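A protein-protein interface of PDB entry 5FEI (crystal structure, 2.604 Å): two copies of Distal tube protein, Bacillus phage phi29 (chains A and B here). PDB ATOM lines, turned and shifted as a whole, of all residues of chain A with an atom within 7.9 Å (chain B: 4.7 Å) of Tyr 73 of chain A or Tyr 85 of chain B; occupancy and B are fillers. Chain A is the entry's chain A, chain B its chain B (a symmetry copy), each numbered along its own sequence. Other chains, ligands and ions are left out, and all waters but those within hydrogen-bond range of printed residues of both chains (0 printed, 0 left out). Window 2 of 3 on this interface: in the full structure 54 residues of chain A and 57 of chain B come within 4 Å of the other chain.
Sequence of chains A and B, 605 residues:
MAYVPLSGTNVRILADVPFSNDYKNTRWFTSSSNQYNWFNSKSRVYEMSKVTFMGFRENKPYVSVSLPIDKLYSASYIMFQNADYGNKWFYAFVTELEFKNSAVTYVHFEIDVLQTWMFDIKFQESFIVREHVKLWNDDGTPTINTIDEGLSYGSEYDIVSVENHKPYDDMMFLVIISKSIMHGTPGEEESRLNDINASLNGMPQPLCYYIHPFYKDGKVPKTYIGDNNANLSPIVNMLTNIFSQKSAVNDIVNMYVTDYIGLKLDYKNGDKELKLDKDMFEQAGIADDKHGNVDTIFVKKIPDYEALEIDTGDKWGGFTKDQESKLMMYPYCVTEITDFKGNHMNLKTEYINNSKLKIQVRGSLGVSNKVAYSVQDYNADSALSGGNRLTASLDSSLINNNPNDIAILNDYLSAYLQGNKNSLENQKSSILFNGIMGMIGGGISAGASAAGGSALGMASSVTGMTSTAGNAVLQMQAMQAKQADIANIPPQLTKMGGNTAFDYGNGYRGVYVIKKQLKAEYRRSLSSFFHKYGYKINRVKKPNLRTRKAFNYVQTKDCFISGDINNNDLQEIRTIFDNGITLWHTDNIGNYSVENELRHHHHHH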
ATOM      1  N   LEU A  14      13.576  -5.347  -8.950  1.00  0.00           N
ATOM      2  CA  LEU A  14      12.646  -4.734  -8.003  1.00  0.00           C
ATOM      3  C   LEU A  14      13.195  -4.658  -6.576  1.00  0.00           C
ATOM      4  O   LEU A  14      14.016  -5.485  -6.162  1.00  0.00           O
ATOM      5  CB  LEU A  14      11.327  -5.520  -7.997  1.00  0.00           C
ATOM      6  CG  LEU A  14      10.754  -5.717  -9.396  1.00  0.00           C
ATOM      7  CD1 LEU A  14       9.445  -6.465  -9.362  1.00  0.00           C
ATOM      8  CD2 LEU A  14      10.593  -4.355 -10.066  1.00  0.00           C
ATOM      9  N   ALA A  15      12.732  -3.652  -5.836  1.00  0.00           N
ATOM     10  CA  ALA A  15      12.977  -3.551  -4.403  1.00  0.00           C
ATOM     11  C   ALA A  15      11.726  -3.969  -3.619  1.00  0.00           C
ATOM     12  O   ALA A  15      10.632  -4.059  -4.187  1.00  0.00           O
ATOM     13  CB  ALA A  15      13.374  -2.138  -4.041  1.00  0.00           C
ATOM     14  N   ASP A  16      11.885  -4.235  -2.325  1.00  0.00           N
ATOM     15  CA  ASP A  16      10.747  -4.357  -1.404  1.00  0.00           C
ATOM     16  C   ASP A  16       9.785  -5.499  -1.684  1.00  0.00           C
ATOM     17  O   ASP A  16       8.588  -5.379  -1.414  1.00  0.00           O
ATOM     18  CB  ASP A  16       9.922  -3.056  -1.389  1.00  0.00           C
ATOM     19  CG  ASP A  16      10.711  -1.854  -0.885  1.00  0.00           C
ATOM     20  OD1 ASP A  16      11.581  -2.038  -0.006  1.00  0.00           O
ATOM     21  OD2 ASP A  16      10.455  -0.722  -1.364  1.00  0.00           O
ATOM     22  N   VAL A  45      14.479  -0.812  -9.376  1.00  0.00           N
ATOM     23  CA  VAL A  45      15.849  -0.449  -9.038  1.00  0.00           C
ATOM     24  C   VAL A  45      16.699  -0.330 -10.301  1.00  0.00           C
ATOM     25  O   VAL A  45      17.623   0.471 -10.371  1.00  0.00           O
ATOM     26  CB  VAL A  45      16.483  -1.491  -8.073  1.00  0.00           C
ATOM     27  CG1 VAL A  45      17.972  -1.248  -7.898  1.00  0.00           C
ATOM     28  CG2 VAL A  45      15.774  -1.474  -6.732  1.00  0.00           C
ATOM     29  N   PRO A  68      27.589  -0.123  -9.246  1.00  0.00           N
ATOM     30  CA  PRO A  68      28.349  -0.485  -8.045  1.00  0.00           C
ATOM     31  C   PRO A  68      27.499  -1.261  -7.044  1.00  0.00           C
ATOM     32  O   PRO A  68      26.343  -0.922  -6.804  1.00  0.00           O
ATOM     33  CB  PRO A  68      28.766   0.874  -7.468  1.00  0.00           C
ATOM     34  CG  PRO A  68      28.746   1.802  -8.645  1.00  0.00           C
ATOM     35  CD  PRO A  68      27.618   1.327  -9.508  1.00  0.00           C
ATOM     36  N   ILE A  69      28.088  -2.297  -6.463  1.00  0.00           N
ATOM     37  CA  ILE A  69      27.386  -3.214  -5.568  1.00  0.00           C
ATOM     38  C   ILE A  69      26.620  -2.532  -4.419  1.00  0.00           C
ATOM     39  O   ILE A  69      25.652  -3.087  -3.904  1.00  0.00           O
ATOM     40  CB  ILE A  69      28.376  -4.230  -4.960  1.00  0.00           C
ATOM     41  CG1 ILE A  69      27.635  -5.316  -4.178  1.00  0.00           C
ATOM     42  CG2 ILE A  69      29.379  -3.522  -4.076  1.00  0.00           C
ATOM     43  CD1 ILE A  69      28.433  -6.590  -3.969  1.00  0.00           C
ATOM     44  N   ASP A  70      27.049  -1.340  -4.013  1.00  0.00           N
ATOM     45  CA  ASP A  70      26.342  -0.617  -2.960  1.00  0.00           C
ATOM     46  C   ASP A  70      24.984  -0.114  -3.450  1.00  0.00           C
ATOM     47  O   ASP A  70      24.047   0.010  -2.659  1.00  0.00           O
ATOM     48  CB  ASP A  70      27.180   0.566  -2.459  1.00  0.00           C
ATOM     49  CG  ASP A  70      27.693   1.449  -3.594  1.00  0.00           C
ATOM     50  OD1 ASP A  70      27.611   1.028  -4.768  1.00  0.00           O
ATOM     51  OD2 ASP A  70      28.180   2.567  -3.313  1.00  0.00           O
ATOM     52  N   LYS A  71      24.894   0.168  -4.753  1.00  0.00           N
ATOM     53  CA  LYS A  71      23.690   0.726  -5.381  1.00  0.00           C
ATOM     54  C   LYS A  71      22.595  -0.309  -5.649  1.00  0.00           C
ATOM     55  O   LYS A  71      21.484   0.044  -6.049  1.00  0.00           O
ATOM     56  CB  LYS A  71      24.044   1.420  -6.696  1.00  0.00           C
ATOM     57  CG  LYS A  71      25.236   2.342  -6.594  1.00  0.00           C
ATOM     58  CD  LYS A  71      25.060   3.394  -5.514  1.00  0.00           C
ATOM     59  CE  LYS A  71      26.263   4.329  -5.486  1.00  0.00           C
ATOM     60  NZ  LYS A  71      26.231   5.255  -4.324  1.00  0.00           N
ATOM     61  N   LEU A  72      22.921  -1.585  -5.469  1.00  0.00           N
ATOM     62  CA  LEU A  72      21.978  -2.658  -5.754  1.00  0.00           C
ATOM     63  C   LEU A  72      21.586  -3.402  -4.501  1.00  0.00           C
ATOM     64  O   LEU A  72      21.122  -4.536  -4.578  1.00  0.00           O
ATOM     65  CB  LEU A  72      22.557  -3.642  -6.771  1.00  0.00           C
ATOM     66  CG  LEU A  72      22.807  -3.084  -8.173  1.00  0.00           C
ATOM     67  CD1 LEU A  72      23.753  -3.980  -8.959  1.00  0.00           C
ATOM     68  CD2 LEU A  72      21.489  -2.953  -8.905  1.00  0.00           C
ATOM     69  N   TYR A  73      21.816  -2.795  -3.340  1.00  0.00           N
ATOM     70  CA  TYR A  73      21.512  -3.477  -2.087  1.00  0.00           C
ATOM     71  C   TYR A  73      20.011  -3.668  -1.925  1.00  0.00           C
ATOM     72  O   TYR A  73      19.578  -4.656  -1.336  1.00  0.00           O
ATOM     73  CB  TYR A  73      22.068  -2.719  -0.877  1.00  0.00           C
ATOM     74  CG  TYR A  73      21.679  -3.353   0.453  1.00  0.00           C
ATOM     75  CD1 TYR A  73      22.538  -4.231   1.111  1.00  0.00           C
ATOM     76  CD2 TYR A  73      20.443  -3.082   1.041  1.00  0.00           C
ATOM     77  CE1 TYR A  73      22.176  -4.810   2.319  1.00  0.00           C
ATOM     78  CE2 TYR A  73      20.073  -3.660   2.240  1.00  0.00           C
ATOM     79  CZ  TYR A  73      20.939  -4.518   2.875  1.00  0.00           C
ATOM     80  OH  TYR A  73      20.552  -5.083   4.066  1.00  0.00           O
ATOM     81  N   SER A  74      19.225  -2.733  -2.461  1.00  0.00           N
ATOM     82  CA  SER A  74      17.760  -2.774  -2.323  1.00  0.00           C
ATOM     83  C   SER A  74      17.126  -3.843  -3.198  1.00  0.00           C
ATOM     84  O   SER A  74      15.944  -4.157  -3.053  1.00  0.00           O
ATOM     85  CB  SER A  74      17.139  -1.417  -2.687  1.00  0.00           C
ATOM     86  OG  SER A  74      17.607  -0.375  -1.856  1.00  0.00           O
ATOM     87  N   ALA A  75      17.921  -4.391  -4.107  1.00  0.00           N
ATOM     88  CA  ALA A  75      17.438  -5.362  -5.066  1.00  0.00           C
ATOM     89  C   ALA A  75      16.993  -6.611  -4.333  1.00  0.00           C
ATOM     90  O   ALA A  75      17.711  -7.107  -3.467  1.00  0.00           O
ATOM     91  CB  ALA A  75      18.519  -5.677  -6.085  1.00  0.00           C
ATOM     92  N   SER A  76      15.804  -7.110  -4.653  1.00  0.00           N
ATOM     93  CA  SER A  76      15.302  -8.311  -3.982  1.00  0.00           C
ATOM     94  C   SER A  76      14.713  -9.311  -4.952  1.00  0.00           C
ATOM     95  O   SER A  76      14.532 -10.471  -4.622  1.00  0.00           O
ATOM     96  CB  SER A  76      14.246  -7.946  -2.951  1.00  0.00           C
ATOM     97  OG  SER A  76      13.095  -7.438  -3.595  1.00  0.00           O
ATOM     98  N   VAL A  94      16.357 -12.195  -6.031  1.00  0.00           N
ATOM     99  CA  VAL A  94      17.763 -11.816  -6.034  1.00  0.00           C
ATOM    100  C   VAL A  94      18.392 -12.454  -4.806  1.00  0.00           C
ATOM    101  O   VAL A  94      17.963 -12.201  -3.675  1.00  0.00           O
ATOM    102  CB  VAL A  94      17.952 -10.295  -6.019  1.00  0.00           C
ATOM    103  CG1 VAL A  94      19.429  -9.936  -5.857  1.00  0.00           C
ATOM    104  CG2 VAL A  94      17.389  -9.696  -7.296  1.00  0.00           C
ATOM    105  N   LEU A  97      24.596 -10.533  -4.430  1.00  0.00           N
ATOM    106  CA  LEU A  97      25.342  -9.625  -5.286  1.00  0.00           C
ATOM    107  C   LEU A  97      26.819 -10.008  -5.269  1.00  0.00           C
ATOM    108  O   LEU A  97      27.423 -10.110  -4.200  1.00  0.00           O
ATOM    109  CB  LEU A  97      25.166  -8.189  -4.805  1.00  0.00           C
ATOM    110  CG  LEU A  97      23.725  -7.726  -4.594  1.00  0.00           C
ATOM    111  CD1 LEU A  97      23.734  -6.380  -3.904  1.00  0.00           C
ATOM    112  CD2 LEU A  97      23.002  -7.626  -5.932  1.00  0.00           C
ATOM    113  N   PRO B   5      27.046  -3.176   3.545  1.00  0.00           N
ATOM    114  CA  PRO B   5      28.254  -3.828   3.015  1.00  0.00           C
ATOM    115  C   PRO B   5      28.975  -2.981   1.947  1.00  0.00           C
ATOM    116  O   PRO B   5      29.301  -3.474   0.868  1.00  0.00           O
ATOM    117  CB  PRO B   5      27.707  -5.134   2.420  1.00  0.00           C
ATOM    118  CG  PRO B   5      26.427  -5.394   3.179  1.00  0.00           C
ATOM    119  CD  PRO B   5      25.850  -4.036   3.444  1.00  0.00           C
ATOM    120  N   ASN B  82      27.741   5.765   5.851  1.00  0.00           N
ATOM    121  CA  ASN B  82      27.840   5.832   4.398  1.00  0.00           C
ATOM    122  C   ASN B  82      27.162   7.064   3.809  1.00  0.00           C
ATOM    123  O   ASN B  82      26.044   7.402   4.201  1.00  0.00           O
ATOM    124  CB  ASN B  82      27.254   4.583   3.758  1.00  0.00           C
ATOM    125  CG  ASN B  82      27.249   4.664   2.251  1.00  0.00           C
ATOM    126  OD1 ASN B  82      26.203   4.574   1.613  1.00  0.00           O
ATOM    127  ND2 ASN B  82      28.425   4.851   1.671  1.00  0.00           N
ATOM    128  N   ALA B  83      27.844   7.731   2.879  1.00  0.00           N
ATOM    129  CA  ALA B  83      27.296   8.915   2.211  1.00  0.00           C
ATOM    130  C   ALA B  83      25.888   8.669   1.640  1.00  0.00           C
ATOM    131  O   ALA B  83      25.075   9.592   1.564  1.00  0.00           O
ATOM    132  CB  ALA B  83      28.233   9.370   1.101  1.00  0.00           C
ATOM    133  N   ASP B  84      25.599   7.419   1.278  1.00  0.00           N
ATOM    134  CA  ASP B  84      24.351   7.063   0.602  1.00  0.00           C
ATOM    135  C   ASP B  84      23.250   6.657   1.567  1.00  0.00           C
ATOM    136  O   ASP B  84      22.109   6.454   1.152  1.00  0.00           O
ATOM    137  CB  ASP B  84      24.568   5.913  -0.389  1.00  0.00           C
ATOM    138  CG  ASP B  84      25.366   6.326  -1.605  1.00  0.00           C
ATOM    139  OD1 ASP B  84      25.050   7.384  -2.196  1.00  0.00           O
ATOM    140  OD2 ASP B  84      26.303   5.586  -1.977  1.00  0.00           O
ATOM    141  N   TYR B  85      23.574   6.525   2.849  1.00  0.00           N
ATOM    142  CA  TYR B  85      22.548   6.141   3.797  1.00  0.00           C
ATOM    143  C   TYR B  85      22.375   7.179   4.898  1.00  0.00           C
ATOM    144  O   TYR B  85      21.941   6.845   5.998  1.00  0.00           O
ATOM    145  CB  TYR B  85      22.914   4.806   4.441  1.00  0.00           C
ATOM    146  CG  TYR B  85      22.586   3.590   3.619  1.00  0.00           C
ATOM    147  CD1 TYR B  85      21.494   2.791   3.923  1.00  0.00           C
ATOM    148  CD2 TYR B  85      23.362   3.254   2.519  1.00  0.00           C
ATOM    149  CE1 TYR B  85      21.196   1.677   3.161  1.00  0.00           C
ATOM    150  CE2 TYR B  85      23.077   2.143   1.754  1.00  0.00           C
ATOM    151  CZ  TYR B  85      21.992   1.360   2.076  1.00  0.00           C
ATOM    152  OH  TYR B  85      21.701   0.255   1.311  1.00  0.00           O
ATOM    153  N   GLY B  86      22.668   8.443   4.603  1.00  0.00           N
ATOM    154  CA  GLY B  86      22.417   9.498   5.569  1.00  0.00           C
ATOM    155  C   GLY B  86      23.300   9.358   6.796  1.00  0.00           C
ATOM    156  O   GLY B  86      24.472   8.980   6.703  1.00  0.00           O
ATOM    157  N   ASN B  87      22.735   9.686   7.954  1.00  0.00           N
ATOM    158  CA  ASN B  87      23.461   9.599   9.214  1.00  0.00           C
ATOM    159  C   ASN B  87      23.339   8.206   9.832  1.00  0.00           C
ATOM    160  O   ASN B  87      23.524   8.040  11.040  1.00  0.00           O
ATOM    161  CB  ASN B  87      22.956  10.654  10.205  1.00  0.00           C
ATOM    162  CG  ASN B  87      23.240  12.076   9.745  1.00  0.00           C
ATOM    163  OD1 ASN B  87      24.244  12.343   9.078  1.00  0.00           O
ATOM    164  ND2 ASN B  87      22.356  13.000  10.110  1.00  0.00           N
ATOM    165  N   LYS B  88      23.050   7.204   9.001  1.00  0.00           N
ATOM    166  CA  LYS B  88      22.893   5.843   9.498  1.00  0.00           C
ATOM    167  C   LYS B  88      24.229   5.212   9.861  1.00  0.00           C
ATOM    168  O   LYS B  88      25.215   5.325   9.132  1.00  0.00           O
ATOM    169  CB  LYS B  88      22.191   4.946   8.482  1.00  0.00           C
ATOM    170  CG  LYS B  88      22.057   3.506   8.981  1.00  0.00           C
ATOM    171  CD  LYS B  88      21.458   2.569   7.938  1.00  0.00           C
ATOM    172  CE  LYS B  88      21.157   1.182   8.517  1.00  0.00           C
ATOM    173  NZ  LYS B  88      20.061   1.187   9.544  1.00  0.00           N
ATOM    174  N   PHE B  90      26.547   1.898  10.677  1.00  0.00           N
ATOM    175  CA  PHE B  90      26.705   0.474  10.425  1.00  0.00           C
ATOM    176  C   PHE B  90      27.633  -0.127  11.473  1.00  0.00           C
ATOM    177  O   PHE B  90      28.648   0.468  11.819  1.00  0.00           O
ATOM    178  CB  PHE B  90      27.232   0.236   9.009  1.00  0.00           C
ATOM    179  CG  PHE B  90      26.291   0.699   7.939  1.00  0.00           C
ATOM    180  CD1 PHE B  90      26.254   2.029   7.558  1.00  0.00           C
ATOM    181  CD2 PHE B  90      25.438  -0.193   7.316  1.00  0.00           C
ATOM    182  CE1 PHE B  90      25.380   2.462   6.572  1.00  0.00           C
ATOM    183  CE2 PHE B  90      24.565   0.230   6.328  1.00  0.00           C
ATOM    184  CZ  PHE B  90      24.537   1.559   5.957  1.00  0.00           C
ATOM    185  N   TRP B 117      20.488  -3.402  11.903  1.00  0.00           N
ATOM    186  CA  TRP B 117      19.118  -3.327  11.407  1.00  0.00           C
ATOM    187  C   TRP B 117      18.092  -3.286  12.547  1.00  0.00           C
ATOM    188  O   TRP B 117      16.898  -3.499  12.328  1.00  0.00           O
ATOM    189  CB  TRP B 117      18.845  -4.507  10.455  1.00  0.00           C
ATOM    190  CG  TRP B 117      19.819  -4.557   9.284  1.00  0.00           C
ATOM    191  CD1 TRP B 117      20.765  -5.521   9.035  1.00  0.00           C
ATOM    192  CD2 TRP B 117      19.966  -3.583   8.241  1.00  0.00           C
ATOM    193  NE1 TRP B 117      21.474  -5.209   7.896  1.00  0.00           N
ATOM    194  CE2 TRP B 117      21.008  -4.024   7.394  1.00  0.00           C
ATOM    195  CE3 TRP B 117      19.319  -2.381   7.942  1.00  0.00           C
ATOM    196  CZ2 TRP B 117      21.412  -3.310   6.275  1.00  0.00           C
ATOM    197  CZ3 TRP B 117      19.719  -1.673   6.824  1.00  0.00           C
ATOM    198  CH2 TRP B 117      20.759  -2.140   6.001  1.00  0.00           C
ATOM    199  N   ILE B 565      15.168  -4.899   4.443  1.00  0.00           N
ATOM    200  CA  ILE B 565      16.423  -5.574   4.698  1.00  0.00           C
ATOM    201  C   ILE B 565      16.573  -6.590   3.615  1.00  0.00           C
ATOM    202  O   ILE B 565      15.576  -7.200   3.226  1.00  0.00           O
ATOM    203  CB  ILE B 565      16.444  -6.290   6.071  1.00  0.00           C
ATOM    204  CG1 ILE B 565      16.150  -5.312   7.200  1.00  0.00           C
ATOM    205  CG2 ILE B 565      17.786  -6.965   6.323  1.00  0.00           C
ATOM    206  CD1 ILE B 565      16.025  -6.000   8.534  1.00  0.00           C
ATOM    207  N   ASN B 566      17.785  -6.789   3.113  1.00  0.00           N
ATOM    208  CA  ASN B 566      17.958  -7.876   2.165  1.00  0.00           C
ATOM    209  C   ASN B 566      17.480  -9.131   2.897  1.00  0.00           C
ATOM    210  O   ASN B 566      17.623  -9.246   4.125  1.00  0.00           O
ATOM    211  CB  ASN B 566      19.411  -7.990   1.675  1.00  0.00           C
ATOM    212  CG  ASN B 566      20.368  -8.436   2.773  1.00  0.00           C
ATOM    213  OD1 ASN B 566      20.755  -9.604   2.836  1.00  0.00           O
ATOM    214  ND2 ASN B 566      20.741  -7.510   3.653  1.00  0.00           N
ATOM    215  N   ASP B 569      19.838 -11.083   5.351  1.00  0.00           N
ATOM    216  CA  ASP B 569      20.046 -10.602   6.717  1.00  0.00           C
ATOM    217  C   ASP B 569      18.802 -10.832   7.548  1.00  0.00           C
ATOM    218  O   ASP B 569      18.869 -11.178   8.736  1.00  0.00           O
ATOM    219  CB  ASP B 569      20.428  -9.127   6.717  1.00  0.00           C
ATOM    220  CG  ASP B 569      21.856  -8.907   6.263  1.00  0.00           C
ATOM    221  OD1 ASP B 569      22.629  -9.893   6.276  1.00  0.00           O
ATOM    222  OD2 ASP B 569      22.195  -7.769   5.867  1.00  0.00           O
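The side-chain carboxylate (OD1) of Asp 84 of chain B is in salt-bridge range of the side-chain amino group (NZ) of Lys 71 of chain A, 3.2 Å away.
OH of Tyr 73 of chain A is in hydrogen-bond range of ND2 of Asn 566 of chain B (2.5 Å).
OD2 of Asp 70 of chain A is in salt-bridge range of NZ of Lys 71 of chain A (3.5 Å).
The backbone NH of Asp 84 of chain B sits close to the side-chain amide oxygen of Asn 82 of chain B (2.9 Å).
The side-chain amide nitrogen (ND2) of Asn 566 of chain B lies within hydrogen-bond range of the side-chain carboxylate (OD2) of Asp 569 of chain B, at 2.7 Å.
The backbone NH (N) of Tyr 85 of chain B lies close to the side-chain amide oxygen (OD1) of Asn 82 of chain B.
The indole nitrogen (NE1) of Trp 117 of chain B lies within hydrogen-bond range of the side-chain carboxylate (OD2) of Asp 569 of chain B, 3.3 Å away.
Among the printed residues, pairs that only touch across the chains: Asp 70 of chain A with Asp 84 of chain B, Tyr 73 of chain A with Pro 5 of chain B, Tyr 73 of chain A with Tyr 85 of chain B, Tyr 73 of chain A with Trp 117 of chain B and Tyr 73 of chain A with Asp 569 of chain B.
Tyr 73 of chain A touches five residues of chain B.
Tyr 85 of chain B touches one residue of chain A.
No residue of chain A comes within 4 Å of Gly 86 of chain B.
Of the printed residues of chain B, Lys 71 of chain A touches Asp 84.
Of the printed residues of chain A, Trp 117 of chain B touches Tyr 73 (3.0 Å).
Printed residues of chain A within 4 Å of Asp 84 of chain B: Asp 70 and Lys 71.
Lys 88 of chain B touches none of the printed residues of chain A.
Ala 83 of chain B touches none of the printed residues of chain A.
The nearest residue of chain B that does not touch Tyr 73 of chain A is Ile 565 of chain B (4.04 Å).
The nearest printed residue of chain B that does not touch Asp 70 of chain A is Tyr 85 of chain B (4.6 Å).
Of the 15 printed residues of chain A, 3 touch a printed residue of chain B.
Hydrophobic or aromatic side chains of chain A that line the printed part of chain B: Tyr 73.
Of the 13 printed residues of chain B, 6 touch a printed residue of chain A.
Hydrophobic or aromatic side chains of chain B within 4 Å of the printed part of chain A: Pro 5, Tyr 85 and Trp 117.
No position is printed for both chains.
Of the 7 pairs that touch across the chains among the printed residues, none has its exchanged pair printed and touching as well.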
